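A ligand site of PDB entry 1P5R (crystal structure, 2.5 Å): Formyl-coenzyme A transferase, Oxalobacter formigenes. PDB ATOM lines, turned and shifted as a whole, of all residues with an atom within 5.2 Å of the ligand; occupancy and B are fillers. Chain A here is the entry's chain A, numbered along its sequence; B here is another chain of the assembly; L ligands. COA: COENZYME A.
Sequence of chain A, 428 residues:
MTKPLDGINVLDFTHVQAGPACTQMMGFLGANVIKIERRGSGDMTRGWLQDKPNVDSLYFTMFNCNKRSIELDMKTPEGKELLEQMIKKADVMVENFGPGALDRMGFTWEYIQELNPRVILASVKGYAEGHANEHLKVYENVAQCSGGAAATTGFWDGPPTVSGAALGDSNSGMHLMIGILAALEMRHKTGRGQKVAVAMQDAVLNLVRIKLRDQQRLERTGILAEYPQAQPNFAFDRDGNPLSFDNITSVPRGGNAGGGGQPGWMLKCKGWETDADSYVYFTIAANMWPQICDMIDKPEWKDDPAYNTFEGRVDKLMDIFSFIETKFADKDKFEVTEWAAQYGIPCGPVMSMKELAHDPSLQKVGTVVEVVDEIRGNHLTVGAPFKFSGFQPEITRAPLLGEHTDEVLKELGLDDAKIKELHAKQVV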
ATOM      1  N   HIS A  15     -18.460 -13.887   2.302  1.00  0.00           N
ATOM      2  CA  HIS A  15     -18.432 -14.393   3.662  1.00  0.00           C
ATOM      3  C   HIS A  15     -19.863 -14.720   4.100  1.00  0.00           C
ATOM      4  O   HIS A  15     -20.843 -14.328   3.456  1.00  0.00           O
ATOM      5  CB  HIS A  15     -17.807 -13.374   4.606  1.00  0.00           C
ATOM      6  CG  HIS A  15     -18.493 -12.040   4.619  1.00  0.00           C
ATOM      7  ND1 HIS A  15     -18.322 -11.121   5.631  1.00  0.00           N
ATOM      8  CD2 HIS A  15     -19.352 -11.471   3.729  1.00  0.00           C
ATOM      9  CE1 HIS A  15     -19.054 -10.048   5.373  1.00  0.00           C
ATOM     10  NE2 HIS A  15     -19.676 -10.239   4.232  1.00  0.00           N
ATOM     11  N   VAL A  16     -19.981 -15.454   5.207  1.00  0.00           N
ATOM     12  CA  VAL A  16     -21.268 -15.850   5.747  1.00  0.00           C
ATOM     13  C   VAL A  16     -21.942 -16.943   4.905  1.00  0.00           C
ATOM     14  O   VAL A  16     -21.371 -18.025   4.713  1.00  0.00           O
ATOM     15  CB  VAL A  16     -22.234 -14.649   5.924  1.00  0.00           C
ATOM     16  CG1 VAL A  16     -23.342 -15.012   6.912  1.00  0.00           C
ATOM     17  CG2 VAL A  16     -21.472 -13.423   6.420  1.00  0.00           C
ATOM     18  N   GLN A  17     -23.128 -16.664   4.365  1.00  0.00           N
ATOM     19  CA  GLN A  17     -23.846 -17.700   3.611  1.00  0.00           C
ATOM     20  C   GLN A  17     -24.206 -17.480   2.138  1.00  0.00           C
ATOM     21  O   GLN A  17     -23.843 -18.303   1.300  1.00  0.00           O
ATOM     22  CB  GLN A  17     -25.106 -18.084   4.405  1.00  0.00           C
ATOM     23  CG  GLN A  17     -25.928 -19.201   3.784  1.00  0.00           C
ATOM     24  CD  GLN A  17     -27.014 -19.737   4.705  1.00  0.00           C
ATOM     25  OE1 GLN A  17     -27.862 -20.516   4.285  1.00  0.00           O
ATOM     26  NE2 GLN A  17     -26.990 -19.321   5.973  1.00  0.00           N
ATOM     27  N   ALA A  18     -24.913 -16.399   1.815  1.00  0.00           N
ATOM     28  CA  ALA A  18     -25.314 -16.096   0.442  1.00  0.00           C
ATOM     29  C   ALA A  18     -24.195 -16.313  -0.565  1.00  0.00           C
ATOM     30  O   ALA A  18     -24.271 -17.215  -1.416  1.00  0.00           O
ATOM     31  CB  ALA A  18     -25.827 -14.662   0.333  1.00  0.00           C
ATOM     32  N   GLY A  19     -23.164 -15.481  -0.487  1.00  0.00           N
ATOM     33  CA  GLY A  19     -22.047 -15.598  -1.400  1.00  0.00           C
ATOM     34  C   GLY A  19     -21.344 -16.933  -1.303  1.00  0.00           C
ATOM     35  O   GLY A  19     -21.155 -17.611  -2.312  1.00  0.00           O
ATOM     36  N   GLU A  37      -9.765 -14.109   2.061  1.00  0.00           N
ATOM     37  CA  GLU A  37     -10.203 -13.786   3.416  1.00  0.00           C
ATOM     38  C   GLU A  37      -9.357 -12.748   4.145  1.00  0.00           C
ATOM     39  O   GLU A  37      -8.251 -12.409   3.722  1.00  0.00           O
ATOM     40  CB  GLU A  37     -10.230 -15.068   4.251  1.00  0.00           C
ATOM     41  CG  GLU A  37     -11.059 -16.183   3.637  1.00  0.00           C
ATOM     42  CD  GLU A  37     -11.109 -17.403   4.520  1.00  0.00           C
ATOM     43  OE1 GLU A  37     -11.631 -17.290   5.656  1.00  0.00           O
ATOM     44  OE2 GLU A  37     -10.634 -18.474   4.084  1.00  0.00           O
ATOM     45  N   ARG A  38      -9.906 -12.247   5.255  1.00  0.00           N
ATOM     46  CA  ARG A  38      -9.238 -11.248   6.070  1.00  0.00           C
ATOM     47  C   ARG A  38      -8.094 -11.848   6.874  1.00  0.00           C
ATOM     48  O   ARG A  38      -8.285 -12.832   7.601  1.00  0.00           O
ATOM     49  CB  ARG A  38     -10.227 -10.594   7.046  1.00  0.00           C
ATOM     50  CG  ARG A  38     -11.426  -9.946   6.365  1.00  0.00           C
ATOM     51  CD  ARG A  38     -12.136  -8.978   7.296  1.00  0.00           C
ATOM     52  NE  ARG A  38     -11.272  -7.856   7.675  1.00  0.00           N
ATOM     53  CZ  ARG A  38     -11.685  -6.750   8.278  1.00  0.00           C
ATOM     54  NH1 ARG A  38     -12.975  -6.607   8.584  1.00  0.00           N
ATOM     55  NH2 ARG A  38     -10.828  -5.797   8.587  1.00  0.00           N
ATOM     56  N   ARG A  39      -6.920 -11.243   6.746  1.00  0.00           N
ATOM     57  CA  ARG A  39      -5.718 -11.704   7.441  1.00  0.00           C
ATOM     58  C   ARG A  39      -5.975 -11.845   8.952  1.00  0.00           C
ATOM     59  O   ARG A  39      -6.463 -10.915   9.593  1.00  0.00           O
ATOM     60  CB  ARG A  39      -4.589 -10.709   7.207  1.00  0.00           C
ATOM     61  CG  ARG A  39      -3.208 -11.335   7.053  1.00  0.00           C
ATOM     62  CD  ARG A  39      -2.139 -10.263   6.959  1.00  0.00           C
ATOM     63  NE  ARG A  39      -2.071  -9.493   8.198  1.00  0.00           N
ATOM     64  CZ  ARG A  39      -1.677  -9.990   9.356  1.00  0.00           C
ATOM     65  NH1 ARG A  39      -1.307 -11.269   9.448  1.00  0.00           N
ATOM     66  NH2 ARG A  39      -1.663  -9.223  10.445  1.00  0.00           N
ATOM     67  N   MET A  44     -16.016 -14.695   8.833  1.00  0.00           N
ATOM     68  CA  MET A  44     -16.558 -14.753  10.187  1.00  0.00           C
ATOM     69  C   MET A  44     -17.295 -16.030  10.567  1.00  0.00           C
ATOM     70  O   MET A  44     -17.637 -16.231  11.726  1.00  0.00           O
ATOM     71  CB  MET A  44     -17.460 -13.538  10.462  1.00  0.00           C
ATOM     72  CG  MET A  44     -18.768 -13.531   9.706  1.00  0.00           C
ATOM     73  SD  MET A  44     -19.659 -11.952   9.868  1.00  0.00           S
ATOM     74  CE  MET A  44     -20.547 -12.217  11.423  1.00  0.00           C
ATOM     75  N   LEU A  72      -5.355 -11.862   2.820  1.00  0.00           N
ATOM     76  CA  LEU A  72      -4.916 -10.610   2.178  1.00  0.00           C
ATOM     77  C   LEU A  72      -5.594  -9.358   2.722  1.00  0.00           C
ATOM     78  O   LEU A  72      -6.818  -9.267   2.704  1.00  0.00           O
ATOM     79  CB  LEU A  72      -5.175 -10.718   0.660  1.00  0.00           C
ATOM     80  CG  LEU A  72      -4.887  -9.547  -0.281  1.00  0.00           C
ATOM     81  CD1 LEU A  72      -3.416  -9.160  -0.206  1.00  0.00           C
ATOM     82  CD2 LEU A  72      -5.250  -9.941  -1.719  1.00  0.00           C
ATOM     83  N   ASP A  73      -4.790  -8.407   3.169  1.00  0.00           N
ATOM     84  CA  ASP A  73      -5.312  -7.149   3.687  1.00  0.00           C
ATOM     85  C   ASP A  73      -5.581  -6.188   2.531  1.00  0.00           C
ATOM     86  O   ASP A  73      -4.649  -5.625   1.964  1.00  0.00           O
ATOM     87  CB  ASP A  73      -4.282  -6.541   4.642  1.00  0.00           C
ATOM     88  CG  ASP A  73      -4.849  -5.421   5.480  1.00  0.00           C
ATOM     89  OD1 ASP A  73      -5.694  -4.680   4.971  1.00  0.00           O
ATOM     90  OD2 ASP A  73      -4.422  -5.300   6.649  1.00  0.00           O
ATOM     91  N   MET A  74      -6.860  -6.003   2.186  1.00  0.00           N
ATOM     92  CA  MET A  74      -7.241  -5.136   1.067  1.00  0.00           C
ATOM     93  C   MET A  74      -7.220  -3.620   1.317  1.00  0.00           C
ATOM     94  O   MET A  74      -7.378  -2.848   0.380  1.00  0.00           O
ATOM     95  CB  MET A  74      -8.608  -5.570   0.544  1.00  0.00           C
ATOM     96  CG  MET A  74      -8.634  -7.035   0.168  1.00  0.00           C
ATOM     97  SD  MET A  74     -10.077  -7.545  -0.769  1.00  0.00           S
ATOM     98  CE  MET A  74     -11.291  -7.745   0.558  1.00  0.00           C
ATOM     99  N   LYS A  75      -7.061  -3.198   2.566  1.00  0.00           N
ATOM    100  CA  LYS A  75      -6.996  -1.759   2.871  1.00  0.00           C
ATOM    101  C   LYS A  75      -5.511  -1.394   2.800  1.00  0.00           C
ATOM    102  O   LYS A  75      -5.038  -0.456   3.446  1.00  0.00           O
ATOM    103  CB  LYS A  75      -7.573  -1.458   4.259  1.00  0.00           C
ATOM    104  CG  LYS A  75      -9.096  -1.614   4.339  1.00  0.00           C
ATOM    105  CD  LYS A  75      -9.648  -1.330   5.729  1.00  0.00           C
ATOM    106  CE  LYS A  75     -11.174  -1.513   5.752  1.00  0.00           C
ATOM    107  NZ  LYS A  75     -11.765  -1.300   7.103  1.00  0.00           N
ATOM    108  N   ASN A  96     -20.122 -10.034  -1.306  1.00  0.00           N
ATOM    109  CA  ASN A  96     -21.291  -9.576  -0.554  1.00  0.00           C
ATOM    110  C   ASN A  96     -20.891  -8.207  -0.011  1.00  0.00           C
ATOM    111  O   ASN A  96     -21.280  -7.166  -0.548  1.00  0.00           O
ATOM    112  CB  ASN A  96     -21.604 -10.446   0.675  1.00  0.00           C
ATOM    113  CG  ASN A  96     -21.576 -11.920   0.377  1.00  0.00           C
ATOM    114  OD1 ASN A  96     -20.505 -12.529   0.315  1.00  0.00           O
ATOM    115  ND2 ASN A  96     -22.745 -12.519   0.207  1.00  0.00           N
ATOM    116  N   PHE A  97     -20.100  -8.244   1.057  1.00  0.00           N
ATOM    117  CA  PHE A  97     -19.600  -7.053   1.727  1.00  0.00           C
ATOM    118  C   PHE A  97     -20.698  -6.055   2.053  1.00  0.00           C
ATOM    119  O   PHE A  97     -21.260  -6.087   3.136  1.00  0.00           O
ATOM    120  CB  PHE A  97     -18.504  -6.402   0.878  1.00  0.00           C
ATOM    121  CG  PHE A  97     -17.199  -7.141   0.897  1.00  0.00           C
ATOM    122  CD1 PHE A  97     -16.265  -6.975  -0.127  1.00  0.00           C
ATOM    123  CD2 PHE A  97     -16.884  -8.011   1.943  1.00  0.00           C
ATOM    124  CE1 PHE A  97     -15.058  -7.646  -0.114  1.00  0.00           C
ATOM    125  CE2 PHE A  97     -15.667  -8.695   1.970  1.00  0.00           C
ATOM    126  CZ  PHE A  97     -14.751  -8.514   0.938  1.00  0.00           C
ATOM    127  N   GLY A  98     -20.993  -5.157   1.128  1.00  0.00           N
ATOM    128  CA  GLY A  98     -22.031  -4.184   1.375  1.00  0.00           C
ATOM    129  C   GLY A  98     -22.374  -3.475   0.097  1.00  0.00           C
ATOM    130  O   GLY A  98     -21.782  -3.765  -0.944  1.00  0.00           O
ATOM    131  N   GLY A 100     -21.612  -0.548  -1.125  1.00  0.00           N
ATOM    132  CA  GLY A 100     -20.430  -0.032  -1.797  1.00  0.00           C
ATOM    133  C   GLY A 100     -19.127  -0.290  -1.073  1.00  0.00           C
ATOM    134  O   GLY A 100     -18.203   0.514  -1.152  1.00  0.00           O
ATOM    135  N   ALA A 101     -19.033  -1.428  -0.383  1.00  0.00           N
ATOM    136  CA  ALA A 101     -17.805  -1.749   0.335  1.00  0.00           C
ATOM    137  C   ALA A 101     -16.673  -1.963  -0.673  1.00  0.00           C
ATOM    138  O   ALA A 101     -15.576  -1.445  -0.500  1.00  0.00           O
ATOM    139  CB  ALA A 101     -17.994  -3.006   1.196  1.00  0.00           C
ATOM    140  N   LEU A 102     -16.967  -2.723  -1.726  1.00  0.00           N
ATOM    141  CA  LEU A 102     -15.997  -3.000  -2.776  1.00  0.00           C
ATOM    142  C   LEU A 102     -15.591  -1.736  -3.519  1.00  0.00           C
ATOM    143  O   LEU A 102     -14.443  -1.588  -3.937  1.00  0.00           O
ATOM    144  CB  LEU A 102     -16.553  -4.013  -3.781  1.00  0.00           C
ATOM    145  CG  LEU A 102     -15.682  -5.224  -4.107  1.00  0.00           C
ATOM    146  CD1 LEU A 102     -16.250  -5.925  -5.328  1.00  0.00           C
ATOM    147  CD2 LEU A 102     -14.241  -4.801  -4.347  1.00  0.00           C
ATOM    148  N   ARG A 104     -15.525   1.393  -2.306  1.00  0.00           N
ATOM    149  CA  ARG A 104     -14.665   2.210  -1.458  1.00  0.00           C
ATOM    150  C   ARG A 104     -13.236   1.698  -1.483  1.00  0.00           C
ATOM    151  O   ARG A 104     -12.295   2.455  -1.243  1.00  0.00           O
ATOM    152  CB  ARG A 104     -15.197   2.228  -0.021  1.00  0.00           C
ATOM    153  CG  ARG A 104     -16.647   2.673   0.088  1.00  0.00           C
ATOM    154  CD  ARG A 104     -17.008   3.096   1.503  1.00  0.00           C
ATOM    155  NE  ARG A 104     -18.452   3.200   1.694  1.00  0.00           N
ATOM    156  CZ  ARG A 104     -19.250   2.163   1.942  1.00  0.00           C
ATOM    157  NH1 ARG A 104     -18.742   0.952   2.049  1.00  0.00           N
ATOM    158  NH2 ARG A 104     -20.557   2.338   2.084  1.00  0.00           N
ATOM    159  N   MET A 105     -13.065   0.422  -1.779  1.00  0.00           N
ATOM    160  CA  MET A 105     -11.739  -0.166  -1.853  1.00  0.00           C
ATOM    161  C   MET A 105     -11.084   0.270  -3.165  1.00  0.00           C
ATOM    162  O   MET A 105      -9.933  -0.055  -3.441  1.00  0.00           O
ATOM    163  CB  MET A 105     -11.802  -1.679  -1.771  1.00  0.00           C
ATOM    164  CG  MET A 105     -12.059  -2.187  -0.347  1.00  0.00           C
ATOM    165  SD  MET A 105     -12.106  -3.976  -0.191  1.00  0.00           S
ATOM    166  CE  MET A 105     -13.867  -4.263  -0.220  1.00  0.00           C
ATOM    167  N   VAL A 124     -24.305 -10.000  -4.243  1.00  0.00           N
ATOM    168  CA  VAL A 124     -25.534 -10.249  -3.510  1.00  0.00           C
ATOM    169  C   VAL A 124     -25.732  -9.020  -2.640  1.00  0.00           C
ATOM    170  O   VAL A 124     -24.814  -8.625  -1.920  1.00  0.00           O
ATOM    171  CB  VAL A 124     -25.432 -11.472  -2.577  1.00  0.00           C
ATOM    172  CG1 VAL A 124     -26.649 -11.524  -1.670  1.00  0.00           C
ATOM    173  CG2 VAL A 124     -25.333 -12.741  -3.396  1.00  0.00           C
ATOM    174  N   LYS A 125     -26.919  -8.431  -2.715  1.00  0.00           N
ATOM    175  CA  LYS A 125     -27.235  -7.235  -1.937  1.00  0.00           C
ATOM    176  C   LYS A 125     -28.495  -7.499  -1.129  1.00  0.00           C
ATOM    177  O   LYS A 125     -29.185  -8.490  -1.348  1.00  0.00           O
ATOM    178  CB  LYS A 125     -27.525  -6.049  -2.871  1.00  0.00           C
ATOM    179  CG  LYS A 125     -26.596  -5.917  -4.058  1.00  0.00           C
ATOM    180  CD  LYS A 125     -27.085  -4.782  -4.972  1.00  0.00           C
ATOM    181  CE  LYS A 125     -26.195  -4.598  -6.201  1.00  0.00           C
ATOM    182  NZ  LYS A 125     -26.712  -3.502  -7.090  1.00  0.00           N
ATOM    183  N   GLY A 126     -28.796  -6.607  -0.194  1.00  0.00           N
ATOM    184  CA  GLY A 126     -29.999  -6.754   0.603  1.00  0.00           C
ATOM    185  C   GLY A 126     -31.174  -6.303  -0.243  1.00  0.00           C
ATOM    186  O   GLY A 126     -32.197  -6.978  -0.323  1.00  0.00           O
ATOM    187  N   LEU A 136     -28.882  -0.518   3.173  1.00  0.00           N
ATOM    188  CA  LEU A 136     -28.949  -1.414   4.319  1.00  0.00           C
ATOM    189  C   LEU A 136     -28.246  -2.767   4.284  1.00  0.00           C
ATOM    190  O   LEU A 136     -28.250  -3.456   3.261  1.00  0.00           O
ATOM    191  CB  LEU A 136     -30.409  -1.629   4.696  1.00  0.00           C
ATOM    192  CG  LEU A 136     -31.131  -0.286   4.742  1.00  0.00           C
ATOM    193  CD1 LEU A 136     -32.561  -0.460   5.218  1.00  0.00           C
ATOM    194  CD2 LEU A 136     -30.362   0.651   5.669  1.00  0.00           C
ATOM    195  N   LYS A 137     -27.651  -3.099   5.424  1.00  0.00           N
ATOM    196  CA  LYS A 137     -26.964  -4.364   5.652  1.00  0.00           C
ATOM    197  C   LYS A 137     -28.082  -5.333   5.984  1.00  0.00           C
ATOM    198  O   LYS A 137     -29.006  -4.997   6.736  1.00  0.00           O
ATOM    199  CB  LYS A 137     -25.980  -4.222   6.828  1.00  0.00           C
ATOM    200  CG  LYS A 137     -24.769  -3.332   6.530  1.00  0.00           C
ATOM    201  CD  LYS A 137     -23.801  -3.260   7.707  1.00  0.00           C
ATOM    202  CE  LYS A 137     -22.566  -2.430   7.344  1.00  0.00           C
ATOM    203  NZ  LYS A 137     -21.589  -2.301   8.472  1.00  0.00           N
ATOM    204  N   VAL A 138     -28.016  -6.538   5.431  1.00  0.00           N
ATOM    205  CA  VAL A 138     -29.074  -7.496   5.644  1.00  0.00           C
ATOM    206  C   VAL A 138     -28.657  -8.920   5.977  1.00  0.00           C
ATOM    207  O   VAL A 138     -27.734  -9.468   5.370  1.00  0.00           O
ATOM    208  CB  VAL A 138     -29.988  -7.554   4.402  1.00  0.00           C
ATOM    209  CG1 VAL A 138     -31.051  -8.610   4.574  1.00  0.00           C
ATOM    210  CG2 VAL A 138     -30.614  -6.189   4.170  1.00  0.00           C
ATOM    211  N   TYR A 139     -29.352  -9.502   6.950  1.00  0.00           N
ATOM    212  CA  TYR A 139     -29.136 -10.875   7.380  1.00  0.00           C
ATOM    213  C   TYR A 139     -30.378 -11.697   7.005  1.00  0.00           C
ATOM    214  O   TYR A 139     -31.456 -11.140   6.724  1.00  0.00           O
ATOM    215  CB  TYR A 139     -28.928 -10.963   8.908  1.00  0.00           C
ATOM    216  CG  TYR A 139     -27.542 -10.599   9.395  1.00  0.00           C
ATOM    217  CD1 TYR A 139     -27.314  -9.408  10.081  1.00  0.00           C
ATOM    218  CD2 TYR A 139     -26.450 -11.464   9.210  1.00  0.00           C
ATOM    219  CE1 TYR A 139     -26.040  -9.070  10.558  1.00  0.00           C
ATOM    220  CE2 TYR A 139     -25.166 -11.137   9.685  1.00  0.00           C
ATOM    221  CZ  TYR A 139     -24.974  -9.947  10.361  1.00  0.00           C
ATOM    222  OH  TYR A 139     -23.728  -9.608  10.852  1.00  0.00           O
ATOM    223  N   GLU A 140     -30.212 -13.016   7.002  1.00  0.00           N
ATOM    224  CA  GLU A 140     -31.237 -14.002   6.668  1.00  0.00           C
ATOM    225  C   GLU A 140     -32.685 -13.654   6.971  1.00  0.00           C
ATOM    226  O   GLU A 140     -33.498 -13.429   6.071  1.00  0.00           O
ATOM    227  CB  GLU A 140     -30.855 -15.342   7.335  1.00  0.00           C
ATOM    228  CG  GLU A 140     -31.841 -16.511   7.166  1.00  0.00           C
ATOM    229  CD  GLU A 140     -32.006 -16.970   5.723  1.00  0.00           C
ATOM    230  OE1 GLU A 140     -31.002 -17.335   5.067  1.00  0.00           O
ATOM    231  OE2 GLU A 140     -33.149 -16.966   5.227  1.00  0.00           O
ATOM    232  N   GLY A 168     -33.409 -16.260   2.465  1.00  0.00           N
ATOM    233  CA  GLY A 168     -32.664 -15.062   2.130  1.00  0.00           C
ATOM    234  C   GLY A 168     -31.201 -15.293   1.782  1.00  0.00           C
ATOM    235  O   GLY A 168     -30.680 -14.650   0.888  1.00  0.00           O
ATOM    236  N   ASP A 169     -30.540 -16.224   2.485  1.00  0.00           N
ATOM    237  CA  ASP A 169     -29.125 -16.492   2.245  1.00  0.00           C
ATOM    238  C   ASP A 169     -28.825 -17.491   1.109  1.00  0.00           C
ATOM    239  O   ASP A 169     -28.564 -17.075  -0.014  1.00  0.00           O
ATOM    240  CB  ASP A 169     -28.473 -16.962   3.546  1.00  0.00           C
ATOM    241  CG  ASP A 169     -28.393 -15.855   4.590  1.00  0.00           C
ATOM    242  OD1 ASP A 169     -28.987 -14.785   4.364  1.00  0.00           O
ATOM    243  OD2 ASP A 169     -27.742 -16.036   5.647  1.00  0.00           O
ATOM    244  N   MET A 200     -31.346  -9.915  -1.979  1.00  0.00           N
ATOM    245  CA  MET A 200     -31.975 -10.926  -1.155  1.00  0.00           C
ATOM    246  C   MET A 200     -33.489 -10.774  -1.117  1.00  0.00           C
ATOM    247  O   MET A 200     -34.225 -11.761  -1.145  1.00  0.00           O
ATOM    248  CB  MET A 200     -31.394 -10.867   0.247  1.00  0.00           C
ATOM    249  CG  MET A 200     -29.903 -11.119   0.269  1.00  0.00           C
ATOM    250  SD  MET A 200     -29.201 -10.901   1.886  1.00  0.00           S
ATOM    251  CE  MET A 200     -29.876 -12.334   2.739  1.00  0.00           C
ATOM    252  N   ASN B 287     -21.179  -7.409  17.141  1.00  0.00           N
ATOM    253  CA  ASN B 287     -20.323  -6.275  16.765  1.00  0.00           C
ATOM    254  C   ASN B 287     -21.019  -4.915  16.836  1.00  0.00           C
ATOM    255  O   ASN B 287     -20.537  -3.928  16.281  1.00  0.00           O
ATOM    256  CB  ASN B 287     -19.769  -6.489  15.358  1.00  0.00           C
ATOM    257  CG  ASN B 287     -19.044  -7.819  15.220  1.00  0.00           C
ATOM    258  OD1 ASN B 287     -18.191  -8.162  16.044  1.00  0.00           O
ATOM    259  ND2 ASN B 287     -19.388  -8.578  14.187  1.00  0.00           N
HETATM  260  N1A COA L   1      -9.477  -6.415   4.181  1.00  0.00           N
HETATM  261  C2A COA L   1      -9.848  -5.108   4.505  1.00  0.00           C
HETATM  262  N3A COA L   1     -11.101  -4.672   4.654  1.00  0.00           N
HETATM  263  C4A COA L   1     -12.046  -5.642   4.465  1.00  0.00           C
HETATM  264  C5A COA L   1     -11.821  -6.978   4.138  1.00  0.00           C
HETATM  265  C6A COA L   1     -10.458  -7.385   3.982  1.00  0.00           C
HETATM  266  N6A COA L   1     -10.088  -8.604   3.679  1.00  0.00           N
HETATM  267  N7A COA L   1     -12.982  -7.656   4.012  1.00  0.00           N
HETATM  268  C8A COA L   1     -13.920  -6.760   4.269  1.00  0.00           C
HETATM  269  N9A COA L   1     -13.433  -5.512   4.545  1.00  0.00           N
HETATM  270  C1B COA L   1     -14.173  -4.271   4.856  1.00  0.00           C
HETATM  271  C2B COA L   1     -15.375  -4.077   3.957  1.00  0.00           C
HETATM  272  O2B COA L   1     -14.984  -3.780   2.600  1.00  0.00           O
HETATM  273  C3B COA L   1     -16.085  -2.939   4.676  1.00  0.00           C
HETATM  274  O3B COA L   1     -15.530  -1.686   4.345  1.00  0.00           O
HETATM  275  P3B COA L   1     -16.303  -0.305   4.371  1.00  0.00           P
HETATM  276  O7A COA L   1     -17.585  -0.478   3.629  1.00  0.00           O
HETATM  277  O8A COA L   1     -15.393   0.655   3.750  1.00  0.00           O
HETATM  278  O9A COA L   1     -16.654  -0.081   5.909  1.00  0.00           O
HETATM  279  C4B COA L   1     -15.889  -3.289   6.154  1.00  0.00           C
HETATM  280  O4B COA L   1     -14.733  -4.199   6.157  1.00  0.00           O
HETATM  281  C5B COA L   1     -17.088  -3.989   6.824  1.00  0.00           C
HETATM  282  O5B COA L   1     -17.460  -5.045   5.959  1.00  0.00           O
HETATM  283  P1A COA L   1     -18.899  -5.730   5.860  1.00  0.00           P
HETATM  284  O1A COA L   1     -18.894  -6.785   4.867  1.00  0.00           O
HETATM  285  O2A COA L   1     -19.998  -4.747   5.537  1.00  0.00           O
HETATM  286  O3A COA L   1     -19.150  -6.348   7.334  1.00  0.00           O
HETATM  287  P2A COA L   1     -20.413  -6.295   8.315  1.00  0.00           P
HETATM  288  O4A COA L   1     -20.928  -4.930   8.465  1.00  0.00           O
HETATM  289  O5A COA L   1     -20.094  -6.956   9.585  1.00  0.00           O
HETATM  290  O6A COA L   1     -21.427  -7.044   7.552  1.00  0.00           O
HETATM  291  CBP COA L   1     -23.192  -8.061   6.722  1.00  0.00           C
HETATM  292  CCP COA L   1     -22.829  -6.936   7.712  1.00  0.00           C
HETATM  293  CDP COA L   1     -24.706  -8.407   6.633  1.00  0.00           C
HETATM  294  CEP COA L   1     -22.418  -9.350   7.099  1.00  0.00           C
HETATM  295  CAP COA L   1     -22.659  -7.530   5.280  1.00  0.00           C
HETATM  296  OAP COA L   1     -21.742  -8.410   4.617  1.00  0.00           O
HETATM  297  C9P COA L   1     -23.792  -7.224   4.232  1.00  0.00           C
HETATM  298  O9P COA L   1     -24.712  -6.270   4.463  1.00  0.00           O
HETATM  299  N8P COA L   1     -23.661  -8.095   3.269  1.00  0.00           N
HETATM  300  C7P COA L   1     -24.545  -8.356   2.084  1.00  0.00           C
HETATM  301  C6P COA L   1     -25.371  -9.305   2.930  1.00  0.00           C
HETATM  302  C5P COA L   1     -25.688 -10.678   2.511  1.00  0.00           C
HETATM  303  O5P COA L   1     -25.310 -11.182   1.440  1.00  0.00           O
HETATM  304  N4P COA L   1     -26.327 -11.293   3.510  1.00  0.00           N
HETATM  305  C3P COA L   1     -26.638 -12.734   3.373  1.00  0.00           C
HETATM  306  C2P COA L   1     -25.544 -13.282   4.306  1.00  0.00           C
HETATM  307  S1P COA L   1     -25.218 -14.968   4.030  1.00  0.00           S
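The backbone carbonyl oxygen (O) of Gly 100 lies close to the guanidinium group (NH1) of Arg 104.
O of Gly 126 sits at hydrogen-bond distance from N of Met 200, 3.5 Å away.
The backbone NH (N) of Asp 169 sits at hydrogen-bond distance from the side-chain carboxylate (OE1) of Glu 140 (2.8 Å).
The side-chain amide nitrogen (ND2) of Asn 96 sits close to the backbone NH (N) of Gly 19, 3.1 Å away.
N of Lys 75 sits at hydrogen-bond distance from OD1 of Asp 73, at 3.1 Å.
O of Lys 125 is in hydrogen-bond range of N of Met 200, 2.7 Å away.
The side-chain carboxylate (OD2) of Asp 169 lies within hydrogen-bond range of the side-chain amide nitrogen (NE2) of Gln 17.
The backbone NH of Leu 72 is in hydrogen-bond range of the backbone carbonyl oxygen of Glu 37, 3.1 Å away.
OD2 of Asp 169 lies close to S1P of the ligand.
A ring nitrogen (NE2) of His 15 lies within hydrogen-bond range of an oxygen (OAP) of the ligand.
N6A of the ligand lies within hydrogen-bond range of O of Leu 72, at 3.5 Å.
The backbone NH of Ala 18 sits close to a sulfur (S1P) of the ligand, at 2.7 Å.
An oxygen (O9P) of the ligand is in hydrogen-bond range of the backbone NH (N) of Val 138 (3.5 Å).
O of Phe 97 sits at hydrogen-bond distance from OAP of the ligand (2.8 Å).
N4P of the ligand sits at hydrogen-bond distance from O of Val 138, 3.0 Å away.
A sulfur (S1P) of the ligand lies close to the backbone NH of Gln 17, at 2.7 Å.
An oxygen (O7A) of the ligand lies within salt-bridge range of the guanidinium group of Arg 104 (2.4 Å).
The side-chain amide nitrogen (ND2) of Asn 96 is in hydrogen-bond range of an oxygen (O5P) of the ligand (3.1 Å).
The side-chain sulfur (SD) of Met 200 lies within hydrogen-bond range of a nitrogen (N4P) of the ligand, at 3.3 Å.
O4A of the ligand lies within salt-bridge range of NZ of Lys 137, 2.7 Å away.
A nitrogen (N1A) of the ligand lies within hydrogen-bond range of the backbone NH (N) of Met 74, at 3.3 Å.
Val 16 touches the ligand.
Arg 38 touches the ligand.
CE of Lys 75 touches N3A of the ligand (3.3 Å).
CB of Ala 101 touches O2B of the ligand (3.4 Å).
Met 105 touches the ligand (CE to O2B, 3.1 Å).
Val 124 touches the ligand.
Tyr 139 touches the ligand (OH to CEP, 3.98 Å).
Hydrophobic or aromatic side chains within 4 Å of the ligand: His 15, Val 16, Ala 18, Met 74, Phe 97, Ala 101, Met 105, Val 124 and Met 200.
Of the 33 residues printed, 19 come within 4 Å of the ligand.
The nearest printed residue that does not touch the ligand is Asp 73 (4.2 Å).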
